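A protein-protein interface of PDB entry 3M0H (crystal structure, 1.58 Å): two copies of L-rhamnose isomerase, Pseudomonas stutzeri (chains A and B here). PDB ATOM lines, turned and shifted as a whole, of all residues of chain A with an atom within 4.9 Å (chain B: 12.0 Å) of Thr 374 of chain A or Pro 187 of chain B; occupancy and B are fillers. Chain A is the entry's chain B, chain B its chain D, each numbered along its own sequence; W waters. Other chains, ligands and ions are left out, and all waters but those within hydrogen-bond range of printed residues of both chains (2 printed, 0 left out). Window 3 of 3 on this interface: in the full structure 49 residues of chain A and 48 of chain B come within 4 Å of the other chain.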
ATOM      1  N   TYR A 300      -8.489   0.213 -35.939  1.00  0.00           N
ATOM      2  CA  TYR A 300      -7.832  -0.717 -35.025  1.00  0.00           C
ATOM      3  C   TYR A 300      -7.834  -2.135 -35.585  1.00  0.00           C
ATOM      4  O   TYR A 300      -6.851  -2.865 -35.447  1.00  0.00           O
ATOM      5  CB  TYR A 300      -8.491  -0.691 -33.643  1.00  0.00           C
ATOM      6  CG  TYR A 300      -7.647  -1.330 -32.554  1.00  0.00           C
ATOM      7  CD1 TYR A 300      -6.279  -1.075 -32.469  1.00  0.00           C
ATOM      8  CD2 TYR A 300      -8.225  -2.158 -31.589  1.00  0.00           C
ATOM      9  CE1 TYR A 300      -5.503  -1.627 -31.448  1.00  0.00           C
ATOM     10  CE2 TYR A 300      -7.454  -2.718 -30.559  1.00  0.00           C
ATOM     11  CZ  TYR A 300      -6.094  -2.445 -30.499  1.00  0.00           C
ATOM     12  OH  TYR A 300      -5.320  -2.976 -29.488  1.00  0.00           O
ATOM     13  N   LEU A 304      -4.759  -4.628 -36.084  1.00  0.00           N
ATOM     14  CA  LEU A 304      -4.697  -5.981 -35.539  1.00  0.00           C
ATOM     15  C   LEU A 304      -4.373  -7.021 -36.614  1.00  0.00           C
ATOM     16  O   LEU A 304      -3.728  -8.032 -36.329  1.00  0.00           O
ATOM     17  CB  LEU A 304      -6.004  -6.318 -34.810  1.00  0.00           C
ATOM     18  CG  LEU A 304      -6.221  -5.462 -33.551  1.00  0.00           C
ATOM     19  CD1 LEU A 304      -7.529  -5.827 -32.868  1.00  0.00           C
ATOM     20  CD2 LEU A 304      -5.051  -5.660 -32.588  1.00  0.00           C
ATOM     21  N   ALA A 370      -3.235 -10.023 -19.192  1.00  0.00           N
ATOM     22  CA  ALA A 370      -4.065  -9.530 -20.286  1.00  0.00           C
ATOM     23  C   ALA A 370      -4.091  -8.017 -20.441  1.00  0.00           C
ATOM     24  O   ALA A 370      -4.070  -7.501 -21.566  1.00  0.00           O
ATOM     25  CB  ALA A 370      -5.486 -10.057 -20.127  1.00  0.00           C
ATOM     26  N   LEU A 371      -4.142  -7.307 -19.318  1.00  0.00           N
ATOM     27  CA  LEU A 371      -4.193  -5.857 -19.359  1.00  0.00           C
ATOM     28  C   LEU A 371      -2.931  -5.253 -19.957  1.00  0.00           C
ATOM     29  O   LEU A 371      -3.014  -4.388 -20.829  1.00  0.00           O
ATOM     30  CB  LEU A 371      -4.442  -5.291 -17.957  1.00  0.00           C
ATOM     31  CG  LEU A 371      -4.573  -3.765 -17.915  1.00  0.00           C
ATOM     32  CD1 LEU A 371      -5.809  -3.363 -17.131  1.00  0.00           C
ATOM     33  CD2 LEU A 371      -3.313  -3.169 -17.304  1.00  0.00           C
ATOM     34  N   MET A 372      -1.764  -5.698 -19.501  1.00  0.00           N
ATOM     35  CA  MET A 372      -0.526  -5.160 -20.053  1.00  0.00           C
ATOM     36  C   MET A 372      -0.270  -5.655 -21.472  1.00  0.00           C
ATOM     37  O   MET A 372       0.376  -4.971 -22.258  1.00  0.00           O
ATOM     38  CB  MET A 372       0.672  -5.491 -19.155  1.00  0.00           C
ATOM     39  CG  MET A 372       0.767  -4.624 -17.901  1.00  0.00           C
ATOM     40  SD  MET A 372       0.675  -2.845 -18.250  1.00  0.00           S
ATOM     41  CE  MET A 372       2.100  -2.628 -19.289  1.00  0.00           C
ATOM     42  N   ALA A 373      -0.770  -6.842 -21.808  1.00  0.00           N
ATOM     43  CA  ALA A 373      -0.588  -7.356 -23.160  1.00  0.00           C
ATOM     44  C   ALA A 373      -1.340  -6.449 -24.133  1.00  0.00           C
ATOM     45  O   ALA A 373      -0.795  -6.023 -25.152  1.00  0.00           O
ATOM     46  CB  ALA A 373      -1.112  -8.790 -23.262  1.00  0.00           C
ATOM     47  N   THR A 374      -2.590  -6.134 -23.807  1.00  0.00           N
ATOM     48  CA  THR A 374      -3.382  -5.286 -24.685  1.00  0.00           C
ATOM     49  C   THR A 374      -2.833  -3.856 -24.717  1.00  0.00           C
ATOM     50  O   THR A 374      -2.862  -3.201 -25.759  1.00  0.00           O
ATOM     51  CB  THR A 374      -4.887  -5.310 -24.274  1.00  0.00           C
ATOM     52  OG1 THR A 374      -5.703  -5.138 -25.442  1.00  0.00           O
ATOM     53  CG2 THR A 374      -5.209  -4.211 -23.271  1.00  0.00           C
ATOM     54  N   GLU A 375      -2.311  -3.381 -23.586  1.00  0.00           N
ATOM     55  CA  GLU A 375      -1.738  -2.035 -23.517  1.00  0.00           C
ATOM     56  C   GLU A 375      -0.449  -1.970 -24.336  1.00  0.00           C
ATOM     57  O   GLU A 375      -0.080  -0.910 -24.843  1.00  0.00           O
ATOM     58  CB  GLU A 375      -1.461  -1.654 -22.058  1.00  0.00           C
ATOM     59  CG  GLU A 375      -0.606  -0.402 -21.854  1.00  0.00           C
ATOM     60  CD  GLU A 375      -1.248   0.880 -22.373  1.00  0.00           C
ATOM     61  OE1 GLU A 375      -2.440   0.861 -22.755  1.00  0.00           O
ATOM     62  OE2 GLU A 375      -0.550   1.917 -22.387  1.00  0.00           O
ATOM     63  N   THR A 376       0.237  -3.102 -24.462  1.00  0.00           N
ATOM     64  CA  THR A 376       1.466  -3.143 -25.244  1.00  0.00           C
ATOM     65  C   THR A 376       1.118  -2.913 -26.717  1.00  0.00           C
ATOM     66  O   THR A 376       1.854  -2.239 -27.440  1.00  0.00           O
ATOM     67  CB  THR A 376       2.201  -4.487 -25.052  1.00  0.00           C
ATOM     68  OG1 THR A 376       2.618  -4.594 -23.685  1.00  0.00           O
ATOM     69  CG2 THR A 376       3.434  -4.565 -25.943  1.00  0.00           C
ATOM     70  N   LEU A 377      -0.007  -3.468 -27.161  1.00  0.00           N
ATOM     71  CA  LEU A 377      -0.436  -3.257 -28.543  1.00  0.00           C
ATOM     72  C   LEU A 377      -0.901  -1.813 -28.700  1.00  0.00           C
ATOM     73  O   LEU A 377      -0.596  -1.156 -29.694  1.00  0.00           O
ATOM     74  CB  LEU A 377      -1.593  -4.188 -28.919  1.00  0.00           C
ATOM     75  CG  LEU A 377      -1.298  -5.674 -29.130  1.00  0.00           C
ATOM     76  CD1 LEU A 377      -2.547  -6.344 -29.696  1.00  0.00           C
ATOM     77  CD2 LEU A 377      -0.130  -5.847 -30.091  1.00  0.00           C
ATOM     78  N   LYS A 378      -1.644  -1.320 -27.714  1.00  0.00           N
ATOM     79  CA  LYS A 378      -2.149   0.044 -27.770  1.00  0.00           C
ATOM     80  C   LYS A 378      -1.051   1.100 -27.802  1.00  0.00           C
ATOM     81  O   LYS A 378      -1.208   2.130 -28.449  1.00  0.00           O
ATOM     82  CB  LYS A 378      -3.094   0.318 -26.595  1.00  0.00           C
ATOM     83  CG  LYS A 378      -4.484  -0.290 -26.754  1.00  0.00           C
ATOM     84  CD  LYS A 378      -5.163   0.212 -28.025  1.00  0.00           C
ATOM     85  CE  LYS A 378      -6.657  -0.077 -28.031  1.00  0.00           C
ATOM     86  NZ  LYS A 378      -7.388   0.814 -27.079  1.00  0.00           N
ATOM     87  N   TYR B 143      -7.429 -18.687 -17.113  1.00  0.00           N
ATOM     88  CA  TYR B 143      -6.792 -18.248 -18.348  1.00  0.00           C
ATOM     89  C   TYR B 143      -6.666 -19.349 -19.394  1.00  0.00           C
ATOM     90  O   TYR B 143      -5.842 -19.258 -20.301  1.00  0.00           O
ATOM     91  CB  TYR B 143      -5.408 -17.677 -18.042  1.00  0.00           C
ATOM     92  CG  TYR B 143      -5.431 -16.500 -17.096  1.00  0.00           C
ATOM     93  CD1 TYR B 143      -6.027 -15.295 -17.467  1.00  0.00           C
ATOM     94  CD2 TYR B 143      -4.857 -16.592 -15.829  1.00  0.00           C
ATOM     95  CE1 TYR B 143      -6.048 -14.205 -16.598  1.00  0.00           C
ATOM     96  CE2 TYR B 143      -4.872 -15.510 -14.953  1.00  0.00           C
ATOM     97  CZ  TYR B 143      -5.469 -14.322 -15.344  1.00  0.00           C
ATOM     98  OH  TYR B 143      -5.482 -13.248 -14.481  1.00  0.00           O
ATOM     99  N   GLY B 183      -9.668 -18.886 -24.779  1.00  0.00           N
ATOM    100  CA  GLY B 183      -9.617 -17.780 -25.712  1.00  0.00           C
ATOM    101  C   GLY B 183      -9.103 -16.558 -24.984  1.00  0.00           C
ATOM    102  O   GLY B 183      -8.451 -16.680 -23.946  1.00  0.00           O
ATOM    103  N   SER B 184      -9.389 -15.379 -25.523  1.00  0.00           N
ATOM    104  CA  SER B 184      -8.949 -14.144 -24.892  1.00  0.00           C
ATOM    105  C   SER B 184     -10.066 -13.116 -24.924  1.00  0.00           C
ATOM    106  O   SER B 184     -10.987 -13.208 -25.738  1.00  0.00           O
ATOM    107  CB  SER B 184      -7.724 -13.586 -25.616  1.00  0.00           C
ATOM    108  OG  SER B 184      -8.017 -13.347 -26.982  1.00  0.00           O
ATOM    109  N   ASN B 185      -9.986 -12.146 -24.023  1.00  0.00           N
ATOM    110  CA  ASN B 185     -10.979 -11.081 -23.960  1.00  0.00           C
ATOM    111  C   ASN B 185     -10.371  -9.785 -24.475  1.00  0.00           C
ATOM    112  O   ASN B 185     -11.075  -8.795 -24.640  1.00  0.00           O
ATOM    113  CB  ASN B 185     -11.473 -10.875 -22.523  1.00  0.00           C
ATOM    114  CG  ASN B 185     -12.513 -11.897 -22.113  1.00  0.00           C
ATOM    115  OD1 ASN B 185     -12.779 -12.849 -22.841  1.00  0.00           O
ATOM    116  ND2 ASN B 185     -13.103 -11.708 -20.939  1.00  0.00           N
ATOM    117  N   PHE B 186      -9.066  -9.794 -24.734  1.00  0.00           N
ATOM    118  CA  PHE B 186      -8.392  -8.595 -25.215  1.00  0.00           C
ATOM    119  C   PHE B 186      -7.370  -8.844 -26.305  1.00  0.00           C
ATOM    120  O   PHE B 186      -6.654  -9.847 -26.289  1.00  0.00           O
ATOM    121  CB  PHE B 186      -7.654  -7.880 -24.074  1.00  0.00           C
ATOM    122  CG  PHE B 186      -8.525  -7.528 -22.913  1.00  0.00           C
ATOM    123  CD1 PHE B 186      -8.692  -8.418 -21.859  1.00  0.00           C
ATOM    124  CD2 PHE B 186      -9.191  -6.310 -22.877  1.00  0.00           C
ATOM    125  CE1 PHE B 186      -9.510  -8.100 -20.779  1.00  0.00           C
ATOM    126  CE2 PHE B 186     -10.014  -5.981 -21.803  1.00  0.00           C
ATOM    127  CZ  PHE B 186     -10.173  -6.880 -20.751  1.00  0.00           C
ATOM    128  N   PRO B 187      -7.300  -7.930 -27.283  1.00  0.00           N
ATOM    129  CA  PRO B 187      -6.321  -8.093 -28.357  1.00  0.00           C
ATOM    130  C   PRO B 187      -4.940  -8.133 -27.697  1.00  0.00           C
ATOM    131  O   PRO B 187      -4.664  -7.351 -26.783  1.00  0.00           O
ATOM    132  CB  PRO B 187      -6.521  -6.830 -29.189  1.00  0.00           C
ATOM    133  CG  PRO B 187      -7.987  -6.591 -29.065  1.00  0.00           C
ATOM    134  CD  PRO B 187      -8.256  -6.850 -27.594  1.00  0.00           C
ATOM    135  N   GLY B 188      -4.086  -9.049 -28.143  1.00  0.00           N
ATOM    136  CA  GLY B 188      -2.751  -9.147 -27.578  1.00  0.00           C
ATOM    137  C   GLY B 188      -2.631 -10.095 -26.400  1.00  0.00           C
ATOM    138  O   GLY B 188      -1.547 -10.623 -26.132  1.00  0.00           O
ATOM    139  N   GLN B 189      -3.734 -10.318 -25.692  1.00  0.00           N
ATOM    140  CA  GLN B 189      -3.717 -11.209 -24.534  1.00  0.00           C
ATOM    141  C   GLN B 189      -3.149 -12.573 -24.901  1.00  0.00           C
ATOM    142  O   GLN B 189      -2.345 -13.143 -24.160  1.00  0.00           O
ATOM    143  CB  GLN B 189      -5.128 -11.379 -23.961  1.00  0.00           C
ATOM    144  CG  GLN B 189      -5.211 -12.389 -22.818  1.00  0.00           C
ATOM    145  CD  GLN B 189      -6.620 -12.577 -22.286  1.00  0.00           C
ATOM    146  OE1 GLN B 189      -6.866 -13.456 -21.453  1.00  0.00           O
ATOM    147  NE2 GLN B 189      -7.549 -11.757 -22.756  1.00  0.00           N
ATOM    148  N   SER B 190      -3.577 -13.095 -26.046  1.00  0.00           N
ATOM    149  CA  SER B 190      -3.112 -14.394 -26.513  1.00  0.00           C
ATOM    150  C   SER B 190      -2.447 -14.273 -27.872  1.00  0.00           C
ATOM    151  O   SER B 190      -2.769 -13.379 -28.657  1.00  0.00           O
ATOM    152  CB  SER B 190      -4.287 -15.373 -26.670  1.00  0.00           C
ATOM    153  OG  SER B 190      -5.018 -15.549 -25.471  1.00  0.00           O
ATOM    154  N   ASN B 191      -1.507 -15.169 -28.143  1.00  0.00           N
ATOM    155  CA  ASN B 191      -0.886 -15.216 -29.454  1.00  0.00           C
ATOM    156  C   ASN B 191      -1.738 -16.311 -30.095  1.00  0.00           C
ATOM    157  O   ASN B 191      -1.671 -17.473 -29.681  1.00  0.00           O
ATOM    158  CB  ASN B 191       0.576 -15.650 -29.361  1.00  0.00           C
ATOM    159  CG  ASN B 191       1.211 -15.811 -30.721  1.00  0.00           C
ATOM    160  OD1 ASN B 191       0.806 -16.668 -31.506  1.00  0.00           O
ATOM    161  ND2 ASN B 191       2.206 -14.980 -31.015  1.00  0.00           N
ATOM    162  N   PHE B 192      -2.565 -15.938 -31.070  1.00  0.00           N
ATOM    163  CA  PHE B 192      -3.465 -16.898 -31.711  1.00  0.00           C
ATOM    164  C   PHE B 192      -2.832 -18.231 -32.092  1.00  0.00           C
ATOM    165  O   PHE B 192      -3.356 -19.297 -31.767  1.00  0.00           O
ATOM    166  CB  PHE B 192      -4.102 -16.308 -32.980  1.00  0.00           C
ATOM    167  CG  PHE B 192      -4.907 -15.052 -32.756  1.00  0.00           C
ATOM    168  CD1 PHE B 192      -5.651 -14.865 -31.594  1.00  0.00           C
ATOM    169  CD2 PHE B 192      -4.949 -14.072 -33.743  1.00  0.00           C
ATOM    170  CE1 PHE B 192      -6.427 -13.716 -31.422  1.00  0.00           C
ATOM    171  CE2 PHE B 192      -5.715 -12.924 -33.585  1.00  0.00           C
ATOM    172  CZ  PHE B 192      -6.459 -12.744 -32.419  1.00  0.00           C
ATOM    173  N   THR B 193      -1.710 -18.171 -32.797  1.00  0.00           N
ATOM    174  CA  THR B 193      -1.053 -19.383 -33.253  1.00  0.00           C
ATOM    175  C   THR B 193      -0.450 -20.228 -32.140  1.00  0.00           C
ATOM    176  O   THR B 193      -0.635 -21.444 -32.122  1.00  0.00           O
ATOM    177  CB  THR B 193       0.011 -19.045 -34.309  1.00  0.00           C
ATOM    178  OG1 THR B 193      -0.639 -18.451 -35.442  1.00  0.00           O
ATOM    179  CG2 THR B 193       0.750 -20.297 -34.760  1.00  0.00           C
ATOM    180  N   ALA B 195      -1.317 -20.342 -29.019  1.00  0.00           N
ATOM    181  CA  ALA B 195      -2.397 -20.907 -28.216  1.00  0.00           C
ATOM    182  C   ALA B 195      -2.984 -22.124 -28.926  1.00  0.00           C
ATOM    183  O   ALA B 195      -3.282 -23.143 -28.297  1.00  0.00           O
ATOM    184  CB  ALA B 195      -3.489 -19.860 -27.980  1.00  0.00           C
ATOM    185  N   ALA B 226     -15.147 -16.479 -23.898  1.00  0.00           N
ATOM    186  CA  ALA B 226     -14.121 -15.559 -24.396  1.00  0.00           C
ATOM    187  C   ALA B 226     -14.787 -14.542 -25.321  1.00  0.00           C
ATOM    188  O   ALA B 226     -15.495 -14.916 -26.262  1.00  0.00           O
ATOM    189  CB  ALA B 226     -13.030 -16.327 -25.134  1.00  0.00           C
ATOM    190  N   PHE B 227     -14.549 -13.258 -25.061  1.00  0.00           N
ATOM    191  CA  PHE B 227     -15.197 -12.203 -25.834  1.00  0.00           C
ATOM    192  C   PHE B 227     -14.396 -11.425 -26.871  1.00  0.00           C
ATOM    193  O   PHE B 227     -14.883 -10.424 -27.406  1.00  0.00           O
ATOM    194  CB  PHE B 227     -15.900 -11.248 -24.864  1.00  0.00           C
ATOM    195  CG  PHE B 227     -16.941 -11.928 -24.014  1.00  0.00           C
ATOM    196  CD1 PHE B 227     -18.034 -12.556 -24.605  1.00  0.00           C
ATOM    197  CD2 PHE B 227     -16.808 -11.975 -22.630  1.00  0.00           C
ATOM    198  CE1 PHE B 227     -18.984 -13.229 -23.828  1.00  0.00           C
ATOM    199  CE2 PHE B 227     -17.748 -12.644 -21.843  1.00  0.00           C
ATOM    200  CZ  PHE B 227     -18.840 -13.274 -22.444  1.00  0.00           C
ATOM    201  N   TYR B 228     -13.171 -11.861 -27.145  1.00  0.00           N
ATOM    202  CA  TYR B 228     -12.378 -11.236 -28.197  1.00  0.00           C
ATOM    203  C   TYR B 228     -11.998 -12.334 -29.187  1.00  0.00           C
ATOM    204  O   TYR B 228     -12.280 -12.228 -30.378  1.00  0.00           O
ATOM    205  CB  TYR B 228     -11.112 -10.553 -27.678  1.00  0.00           C
ATOM    206  CG  TYR B 228     -10.210 -10.170 -28.831  1.00  0.00           C
ATOM    207  CD1 TYR B 228     -10.657  -9.306 -29.836  1.00  0.00           C
ATOM    208  CD2 TYR B 228      -8.964 -10.767 -28.985  1.00  0.00           C
ATOM    209  CE1 TYR B 228      -9.883  -9.059 -30.972  1.00  0.00           C
ATOM    210  CE2 TYR B 228      -8.185 -10.531 -30.111  1.00  0.00           C
ATOM    211  CZ  TYR B 228      -8.651  -9.683 -31.101  1.00  0.00           C
ATOM    212  OH  TYR B 228      -7.895  -9.502 -32.231  1.00  0.00           O
ATOM    213  N   SER B 229     -11.343 -13.385 -28.696  1.00  0.00           N
ATOM    214  CA  SER B 229     -10.984 -14.512 -29.552  1.00  0.00           C
ATOM    215  C   SER B 229     -11.216 -15.816 -28.800  1.00  0.00           C
ATOM    216  O   SER B 229     -11.196 -15.854 -27.571  1.00  0.00           O
ATOM    217  CB  SER B 229      -9.518 -14.439 -30.009  1.00  0.00           C
ATOM    218  OG  SER B 229      -8.637 -15.030 -29.064  1.00  0.00           O
ATOM    219  N   THR B 230     -11.460 -16.876 -29.560  1.00  0.00           N
ATOM    220  CA  THR B 230     -11.683 -18.205 -29.010  1.00  0.00           C
ATOM    221  C   THR B 230     -10.791 -19.132 -29.825  1.00  0.00           C
ATOM    222  O   THR B 230     -10.724 -19.015 -31.049  1.00  0.00           O
ATOM    223  CB  THR B 230     -13.170 -18.613 -29.132  1.00  0.00           C
ATOM    224  OG1 THR B 230     -13.954 -17.821 -28.230  1.00  0.00           O
ATOM    225  CG2 THR B 230     -13.359 -20.084 -28.790  1.00  0.00           C
HETATM  226  O   HOH W   1      -2.082 -12.278 -21.435  1.00  0.00           O
HETATM  227  O   HOH W   2      -4.682 -10.799 -16.516  1.00  0.00           O
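O of Pro 187 of chain B lies within hydrogen-bond range of OG1 of Thr 374 of chain A.
The backbone carbonyl oxygen of Ser 184 of chain B is in hydrogen-bond range of the backbone NH of Tyr 228 of chain B (2.9 Å).
The backbone NH (N) of Asn 185 of chain B lies close to the side-chain amide nitrogen (NE2) of Gln 189 of chain B (2.8 Å).
The side-chain amide nitrogen of Gln 189 of chain B lies close to the backbone NH of Phe 186 of chain B (3.2 Å).
Leu 304 of chain A touches Pro 187 of chain B.
OH of Tyr 228 of chain B touches CD1 of Leu 304 of chain A (3.7 Å).
Ala 370 of chain A touches Phe 186 of chain B (CB to CD1, 3.996 Å).
CB of Ala 370 of chain A touches CD of Gln 189 of chain B, at 3.5 Å.
O of Gly 188 of chain B touches CB of Ala 373 of chain A, 3.4 Å away.
CB of Ala 373 of chain A touches CA of Gln 189 of chain B, at 3.8 Å.
Phe 186 of chain B touches Thr 374 of chain A.
CD1 of Leu 377 of chain A touches C of Pro 187 of chain B, 3.6 Å away.
Gly 188 of chain B touches Leu 377 of chain A (N to CD1, 3.5 Å).
Thr 374 of chain A touches just these residues of chain B: Phe 186 and Pro 187.
Pro 187 of chain B touches just these residues of chain A: Leu 304, Thr 374 and Leu 377.
Of chain B, only Pro 187 (3.9 Å) and Tyr 228 (3.7 Å) come within 4 Å of Leu 304 of chain A.
Leu 371 of chain A touches none of the printed residues of chain B.
No residue of chain B comes within 4 Å of Met 372 of chain A.
No residue of chain B comes within 4 Å of Glu 375 of chain A.
No residue of chain B comes within 4 Å of Thr 376 of chain A.
Leu 377 of chain A touches just these residues of chain B: Pro 187 (3.6 Å) and Gly 188 (3.5 Å).
No residue of chain B comes within 4 Å of Lys 378 of chain A.
Printed residues of chain A within 4 Å of Phe 186 of chain B: Ala 370 (3.996 Å) and Thr 374 (3.6 Å).
Of the printed residues of chain A, Gly 188 of chain B touches Ala 373 (3.4 Å) and Leu 377 (3.5 Å).
Of the printed residues of chain A, Gln 189 of chain B touches Ala 370 and Ala 373.
Printed residues of chain A within 4 Å of Tyr 228 of chain B: Leu 304.
The nearest printed residue of chain B that does not touch Thr 374 of chain A is Gln 189 of chain B (4.7 Å).
The nearest residue of chain A that does not touch Pro 187 of chain B is Tyr 300 of chain A (4.05 Å).
Hydrophobic or aromatic side chains of chain A that line the printed part of chain B: Leu 304, Ala 370, Ala 373 and Leu 377.
Printed residues of chain B that touch a printed residue of chain A: Phe 186, Pro 187, Gly 188, Gln 189 and Tyr 228.
Among the printed residues, 10 pairs touch across the chains.
No position is printed for both chains.
Of the 10 pairs that touch across the chains among the printed residues, none has its exchanged pair printed and touching as well.
Water W1 bridges O of Gln 189 of chain B (2.9 Å) and N of Ala 370 of chain A (3.4 Å).
Water W2 bridges N of Ala 370 of chain A (3.1 Å) and OH of Tyr 143 of chain B (3.3 Å).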
